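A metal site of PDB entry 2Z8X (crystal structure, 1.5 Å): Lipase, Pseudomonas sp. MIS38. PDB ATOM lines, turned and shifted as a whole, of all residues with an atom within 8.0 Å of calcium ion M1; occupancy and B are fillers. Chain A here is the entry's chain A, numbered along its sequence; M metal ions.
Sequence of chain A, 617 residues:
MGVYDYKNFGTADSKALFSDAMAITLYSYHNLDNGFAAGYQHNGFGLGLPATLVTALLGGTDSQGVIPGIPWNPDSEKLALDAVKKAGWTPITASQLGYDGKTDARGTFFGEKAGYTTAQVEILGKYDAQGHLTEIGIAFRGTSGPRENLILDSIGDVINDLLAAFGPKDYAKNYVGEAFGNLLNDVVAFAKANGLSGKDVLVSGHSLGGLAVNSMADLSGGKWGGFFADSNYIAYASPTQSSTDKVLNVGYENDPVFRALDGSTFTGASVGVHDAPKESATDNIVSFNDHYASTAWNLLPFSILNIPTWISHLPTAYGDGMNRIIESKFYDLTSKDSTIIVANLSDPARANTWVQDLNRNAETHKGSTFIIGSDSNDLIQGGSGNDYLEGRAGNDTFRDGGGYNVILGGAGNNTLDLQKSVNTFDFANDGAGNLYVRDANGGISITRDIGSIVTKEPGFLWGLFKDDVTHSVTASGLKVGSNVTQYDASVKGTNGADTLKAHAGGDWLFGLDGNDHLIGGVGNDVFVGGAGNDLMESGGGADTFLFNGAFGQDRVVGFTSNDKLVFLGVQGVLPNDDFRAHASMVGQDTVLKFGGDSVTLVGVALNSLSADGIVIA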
ATOM      1  N   ALA A 502     -19.736 -10.866  16.896  1.00  0.00           N
ATOM      2  CA  ALA A 502     -19.207  -9.970  17.915  1.00  0.00           C
ATOM      3  C   ALA A 502     -17.702 -10.149  18.056  1.00  0.00           C
ATOM      4  O   ALA A 502     -17.175 -11.248  17.886  1.00  0.00           O
ATOM      5  CB  ALA A 502     -19.859 -10.230  19.273  1.00  0.00           C
ATOM      6  N   HIS A 503     -17.019  -9.058  18.387  1.00  0.00           N
ATOM      7  CA  HIS A 503     -15.605  -9.116  18.727  1.00  0.00           C
ATOM      8  C   HIS A 503     -15.485  -9.532  20.172  1.00  0.00           C
ATOM      9  O   HIS A 503     -16.457  -9.459  20.948  1.00  0.00           O
ATOM     10  CB  HIS A 503     -14.930  -7.759  18.481  1.00  0.00           C
ATOM     11  CG  HIS A 503     -15.051  -7.282  17.066  1.00  0.00           C
ATOM     12  ND1 HIS A 503     -16.073  -6.480  16.633  1.00  0.00           N
ATOM     13  CD2 HIS A 503     -14.289  -7.529  15.975  1.00  0.00           C
ATOM     14  CE1 HIS A 503     -15.935  -6.231  15.343  1.00  0.00           C
ATOM     15  NE2 HIS A 503     -14.858  -6.851  14.917  1.00  0.00           N
ATOM     16  N   ALA A 504     -14.283  -9.949  20.570  1.00  0.00           N
ATOM     17  CA  ALA A 504     -14.057 -10.495  21.904  1.00  0.00           C
ATOM     18  C   ALA A 504     -14.403  -9.505  23.016  1.00  0.00           C
ATOM     19  O   ALA A 504     -14.806  -9.919  24.098  1.00  0.00           O
ATOM     20  CB  ALA A 504     -12.606 -10.970  22.045  1.00  0.00           C
ATOM     21  N   GLY A 506     -16.870  -7.548  23.233  1.00  0.00           N
ATOM     22  CA  GLY A 506     -18.317  -7.379  23.396  1.00  0.00           C
ATOM     23  C   GLY A 506     -18.885  -6.352  22.450  1.00  0.00           C
ATOM     24  O   GLY A 506     -18.297  -5.281  22.253  1.00  0.00           O
ATOM     25  N   ASP A 507     -20.029  -6.667  21.857  1.00  0.00           N
ATOM     26  CA  ASP A 507     -20.663  -5.767  20.886  1.00  0.00           C
ATOM     27  C   ASP A 507     -22.172  -5.763  21.055  1.00  0.00           C
ATOM     28  O   ASP A 507     -22.765  -6.763  21.458  1.00  0.00           O
ATOM     29  CB  ASP A 507     -20.371  -6.225  19.453  1.00  0.00           C
ATOM     30  CG  ASP A 507     -19.028  -5.764  18.912  1.00  0.00           C
ATOM     31  OD1 ASP A 507     -18.761  -4.542  18.885  1.00  0.00           O
ATOM     32  OD2 ASP A 507     -18.238  -6.630  18.475  1.00  0.00           O
ATOM     33  N   LEU A 509     -25.172  -6.201  18.824  1.00  0.00           N
ATOM     34  CA  LEU A 509     -25.382  -6.810  17.515  1.00  0.00           C
ATOM     35  C   LEU A 509     -26.787  -6.461  17.033  1.00  0.00           C
ATOM     36  O   LEU A 509     -27.781  -6.881  17.635  1.00  0.00           O
ATOM     37  CB  LEU A 509     -25.184  -8.333  17.568  1.00  0.00           C
ATOM     38  CG  LEU A 509     -23.807  -8.863  17.986  1.00  0.00           C
ATOM     39  CD1 LEU A 509     -23.808 -10.380  18.043  1.00  0.00           C
ATOM     40  CD2 LEU A 509     -22.734  -8.380  17.025  1.00  0.00           C
ATOM     41  N   ILE A 519     -23.710 -14.123  16.151  1.00  0.00           N
ATOM     42  CA  ILE A 519     -22.726 -14.958  16.834  1.00  0.00           C
ATOM     43  C   ILE A 519     -22.014 -14.102  17.866  1.00  0.00           C
ATOM     44  O   ILE A 519     -21.135 -13.317  17.535  1.00  0.00           O
ATOM     45  CB  ILE A 519     -21.702 -15.562  15.849  1.00  0.00           C
ATOM     46  CG1 ILE A 519     -22.411 -16.281  14.700  1.00  0.00           C
ATOM     47  CG2 ILE A 519     -20.752 -16.522  16.570  1.00  0.00           C
ATOM     48  CD1 ILE A 519     -21.456 -16.700  13.582  1.00  0.00           C
ATOM     49  N   GLY A 520     -22.420 -14.247  19.120  1.00  0.00           N
ATOM     50  CA  GLY A 520     -21.761 -13.538  20.200  1.00  0.00           C
ATOM     51  C   GLY A 520     -20.353 -14.084  20.436  1.00  0.00           C
ATOM     52  O   GLY A 520     -19.975 -15.131  19.920  1.00  0.00           O
ATOM     53  N   GLY A 521     -19.577 -13.339  21.211  1.00  0.00           N
ATOM     54  CA  GLY A 521     -18.242 -13.793  21.599  1.00  0.00           C
ATOM     55  C   GLY A 521     -18.152 -13.986  23.097  1.00  0.00           C
ATOM     56  O   GLY A 521     -19.169 -14.009  23.797  1.00  0.00           O
ATOM     57  N   VAL A 522     -16.925 -14.116  23.581  1.00  0.00           N
ATOM     58  CA  VAL A 522     -16.686 -14.367  24.991  1.00  0.00           C
ATOM     59  C   VAL A 522     -16.992 -13.139  25.843  1.00  0.00           C
ATOM     60  O   VAL A 522     -17.027 -13.216  27.075  1.00  0.00           O
ATOM     61  CB  VAL A 522     -15.220 -14.823  25.250  1.00  0.00           C
ATOM     62  CG1 VAL A 522     -14.925 -16.093  24.468  1.00  0.00           C
ATOM     63  CG2 VAL A 522     -14.233 -13.720  24.875  1.00  0.00           C
ATOM     64  N   GLY A 523     -17.180 -11.998  25.185  1.00  0.00           N
ATOM     65  CA  GLY A 523     -17.469 -10.748  25.854  1.00  0.00           C
ATOM     66  C   GLY A 523     -18.943 -10.557  26.124  1.00  0.00           C
ATOM     67  O   GLY A 523     -19.756 -11.398  25.752  1.00  0.00           O
ATOM     68  N   ASN A 524     -19.269  -9.442  26.762  1.00  0.00           N
ATOM     69  CA  ASN A 524     -20.623  -9.098  27.124  1.00  0.00           C
ATOM     70  C   ASN A 524     -21.279  -8.406  25.951  1.00  0.00           C
ATOM     71  O   ASN A 524     -20.973  -7.254  25.630  1.00  0.00           O
ATOM     72  CB  ASN A 524     -20.625  -8.193  28.353  1.00  0.00           C
ATOM     73  CG  ASN A 524     -20.022  -8.865  29.583  1.00  0.00           C
ATOM     74  OD1 ASN A 524     -19.795 -10.068  29.616  1.00  0.00           O
ATOM     75  ND2 ASN A 524     -19.772  -8.061  30.619  1.00  0.00           N
ATOM     76  N   ASP A 525     -22.183  -9.124  25.303  1.00  0.00           N
ATOM     77  CA  ASP A 525     -22.845  -8.662  24.087  1.00  0.00           C
ATOM     78  C   ASP A 525     -24.281  -8.263  24.370  1.00  0.00           C
ATOM     79  O   ASP A 525     -24.891  -8.749  25.321  1.00  0.00           O
ATOM     80  CB  ASP A 525     -22.830  -9.763  23.027  1.00  0.00           C
ATOM     81  CG  ASP A 525     -21.446 -10.330  22.786  1.00  0.00           C
ATOM     82  OD1 ASP A 525     -20.521  -9.539  22.479  1.00  0.00           O
ATOM     83  OD2 ASP A 525     -21.289 -11.567  22.886  1.00  0.00           O
ATOM     84  N   VAL A 526     -24.820  -7.368  23.541  1.00  0.00           N
ATOM     85  CA  VAL A 526     -26.260  -7.071  23.584  1.00  0.00           C
ATOM     86  C   VAL A 526     -26.832  -7.471  22.226  1.00  0.00           C
ATOM     87  O   VAL A 526     -26.418  -6.941  21.205  1.00  0.00           O
ATOM     88  CB  VAL A 526     -26.540  -5.578  23.890  1.00  0.00           C
ATOM     89  CG1 VAL A 526     -28.024  -5.327  23.950  1.00  0.00           C
ATOM     90  CG2 VAL A 526     -25.866  -5.153  25.196  1.00  0.00           C
ATOM     91  N   PHE A 527     -27.744  -8.434  22.233  1.00  0.00           N
ATOM     92  CA  PHE A 527     -28.326  -8.964  21.003  1.00  0.00           C
ATOM     93  C   PHE A 527     -29.656  -8.303  20.715  1.00  0.00           C
ATOM     94  O   PHE A 527     -30.586  -8.396  21.524  1.00  0.00           O
ATOM     95  CB  PHE A 527     -28.567 -10.464  21.133  1.00  0.00           C
ATOM     96  CG  PHE A 527     -27.325 -11.286  21.282  1.00  0.00           C
ATOM     97  CD1 PHE A 527     -26.798 -11.969  20.185  1.00  0.00           C
ATOM     98  CD2 PHE A 527     -26.713 -11.418  22.524  1.00  0.00           C
ATOM     99  CE1 PHE A 527     -25.664 -12.760  20.315  1.00  0.00           C
ATOM    100  CE2 PHE A 527     -25.572 -12.208  22.667  1.00  0.00           C
ATOM    101  CZ  PHE A 527     -25.043 -12.873  21.545  1.00  0.00           C
ATOM    102  N   GLU A 537     -26.510 -16.553  19.437  1.00  0.00           N
ATOM    103  CA  GLU A 537     -25.636 -17.443  20.193  1.00  0.00           C
ATOM    104  C   GLU A 537     -24.797 -16.616  21.162  1.00  0.00           C
ATOM    105  O   GLU A 537     -24.035 -15.768  20.744  1.00  0.00           O
ATOM    106  CB  GLU A 537     -24.727 -18.206  19.225  1.00  0.00           C
ATOM    107  CG  GLU A 537     -25.488 -19.072  18.242  1.00  0.00           C
ATOM    108  CD  GLU A 537     -24.649 -19.477  17.056  1.00  0.00           C
ATOM    109  OE1 GLU A 537     -23.399 -19.352  17.097  1.00  0.00           O
ATOM    110  OE2 GLU A 537     -25.260 -19.947  16.076  1.00  0.00           O
ATOM    111  N   SER A 538     -24.934 -16.877  22.460  1.00  0.00           N
ATOM    112  CA  SER A 538     -24.247 -16.086  23.475  1.00  0.00           C
ATOM    113  C   SER A 538     -22.729 -16.009  23.258  1.00  0.00           C
ATOM    114  O   SER A 538     -22.135 -14.919  23.263  1.00  0.00           O
ATOM    115  CB  SER A 538     -24.540 -16.655  24.873  1.00  0.00           C
ATOM    116  OG  SER A 538     -23.573 -16.211  25.818  1.00  0.00           O
ATOM    117  N   GLY A 539     -22.103 -17.164  23.097  1.00  0.00           N
ATOM    118  CA  GLY A 539     -20.651 -17.209  22.942  1.00  0.00           C
ATOM    119  C   GLY A 539     -19.868 -17.093  24.254  1.00  0.00           C
ATOM    120  O   GLY A 539     -18.640 -17.170  24.237  1.00  0.00           O
ATOM    121  N   GLY A 540     -20.564 -16.922  25.371  1.00  0.00           N
ATOM    122  CA  GLY A 540     -19.923 -16.704  26.679  1.00  0.00           C
ATOM    123  C   GLY A 540     -20.179 -15.295  27.190  1.00  0.00           C
ATOM    124  O   GLY A 540     -20.754 -14.466  26.493  1.00  0.00           O
ATOM    125  N   GLY A 541     -19.769 -15.026  28.421  1.00  0.00           N
ATOM    126  CA  GLY A 541     -19.904 -13.696  28.994  1.00  0.00           C
ATOM    127  C   GLY A 541     -21.271 -13.474  29.605  1.00  0.00           C
ATOM    128  O   GLY A 541     -22.067 -14.417  29.735  1.00  0.00           O
ATOM    129  N   ALA A 542     -21.529 -12.235  29.998  1.00  0.00           N
ATOM    130  CA  ALA A 542     -22.812 -11.829  30.560  1.00  0.00           C
ATOM    131  C   ALA A 542     -23.541 -11.014  29.505  1.00  0.00           C
ATOM    132  O   ALA A 542     -23.273  -9.825  29.305  1.00  0.00           O
ATOM    133  CB  ALA A 542     -22.602 -11.024  31.845  1.00  0.00           C
ATOM    134  N   ASP A 543     -24.449 -11.688  28.793  1.00  0.00           N
ATOM    135  CA  ASP A 543     -25.104 -11.141  27.618  1.00  0.00           C
ATOM    136  C   ASP A 543     -26.526 -10.690  27.899  1.00  0.00           C
ATOM    137  O   ASP A 543     -27.183 -11.191  28.811  1.00  0.00           O
ATOM    138  CB  ASP A 543     -25.119 -12.187  26.491  1.00  0.00           C
ATOM    139  CG  ASP A 543     -23.716 -12.520  25.962  1.00  0.00           C
ATOM    140  OD1 ASP A 543     -22.802 -11.682  26.078  1.00  0.00           O
ATOM    141  OD2 ASP A 543     -23.542 -13.607  25.390  1.00  0.00           O
ATOM    142  N   THR A 544     -27.003  -9.756  27.077  1.00  0.00           N
ATOM    143  CA  THR A 544     -28.349  -9.228  27.143  1.00  0.00           C
ATOM    144  C   THR A 544     -29.008  -9.481  25.798  1.00  0.00           C
ATOM    145  O   THR A 544     -28.386  -9.267  24.773  1.00  0.00           O
ATOM    146  CB  THR A 544     -28.308  -7.699  27.413  1.00  0.00           C
ATOM    147  OG1 THR A 544     -27.582  -7.455  28.622  1.00  0.00           O
ATOM    148  CG2 THR A 544     -29.709  -7.124  27.512  1.00  0.00           C
ATOM    149  N   PHE A 545     -30.247  -9.984  25.822  1.00  0.00           N
ATOM    150  CA  PHE A 545     -31.023 -10.203  24.598  1.00  0.00           C
ATOM    151  C   PHE A 545     -32.261  -9.328  24.705  1.00  0.00           C
ATOM    152  O   PHE A 545     -33.041  -9.466  25.647  1.00  0.00           O
ATOM    153  CB  PHE A 545     -31.415 -11.679  24.469  1.00  0.00           C
ATOM    154  CG  PHE A 545     -30.232 -12.628  24.432  1.00  0.00           C
ATOM    155  CD1 PHE A 545     -29.779 -13.153  23.215  1.00  0.00           C
ATOM    156  CD2 PHE A 545     -29.574 -12.982  25.605  1.00  0.00           C
ATOM    157  CE1 PHE A 545     -28.683 -14.031  23.178  1.00  0.00           C
ATOM    158  CE2 PHE A 545     -28.482 -13.865  25.587  1.00  0.00           C
ATOM    159  CZ  PHE A 545     -28.035 -14.370  24.364  1.00  0.00           C
ATOM    160  N   GLY A 558     -27.067 -20.908  24.285  1.00  0.00           N
ATOM    161  CA  GLY A 558     -26.017 -20.645  25.260  1.00  0.00           C
ATOM    162  C   GLY A 558     -26.420 -19.744  26.404  1.00  0.00           C
ATOM    163  O   GLY A 558     -25.545 -19.151  27.049  1.00  0.00           O
ATOM    164  N   ASP A 563     -26.915 -14.185  32.199  1.00  0.00           N
ATOM    165  CA  ASP A 563     -27.465 -13.490  31.044  1.00  0.00           C
ATOM    166  C   ASP A 563     -28.870 -12.957  31.345  1.00  0.00           C
ATOM    167  O   ASP A 563     -29.488 -13.312  32.357  1.00  0.00           O
ATOM    168  CB  ASP A 563     -27.475 -14.391  29.814  1.00  0.00           C
ATOM    169  CG  ASP A 563     -26.111 -14.980  29.528  1.00  0.00           C
ATOM    170  OD1 ASP A 563     -25.106 -14.235  29.595  1.00  0.00           O
ATOM    171  OD2 ASP A 563     -26.028 -16.187  29.230  1.00  0.00           O
HETATM  172 CA    CA M   1     -21.194 -13.097  24.684  1.00  0.00          CA
HETATM  173 CA    CA M   2     -23.640 -16.146  30.169  1.00  0.00          CA
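Within 4 Å of calcium ion M1: Gly 521, Gly 523, Asp 525, Ser 538, Gly 540 and Asp 543. The nearest printed residue that does not touch calcium ion M1 is Gly 539 (4.2 Å).
O of Gly 540 binds calcium ion M1, at 2.3 Å. Calcium ion M1 is bound by the side-chain carboxylate (OD2) of Asp 525, 2.4 Å away. O of Gly 521 binds calcium ion M1 (2.4 Å). Calcium ion M1 is bound by O of Gly 523, at 2.5 Å. O of Ser 538 is bound to calcium ion M1, at 2.5 Å. OD2 of Asp 543 is bound to calcium ion M1 (2.5 Å). OD1 of Asp 543 is bound to calcium ion M1 (2.6 Å).
N of Gly 540 is in hydrogen-bond range of OG of Ser 538 (3.1 Å). N of Thr 544 lies within hydrogen-bond range of O of Asp 525 (2.9 Å). OD1 of Asp 525 sits at hydrogen-bond distance from N of Asp 507, 3.0 Å away. N of Gly 523 lies close to O of Ala 504 (3.3 Å). OD1 of Asp 563 sits close to N of Asp 543, at 2.7 Å.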
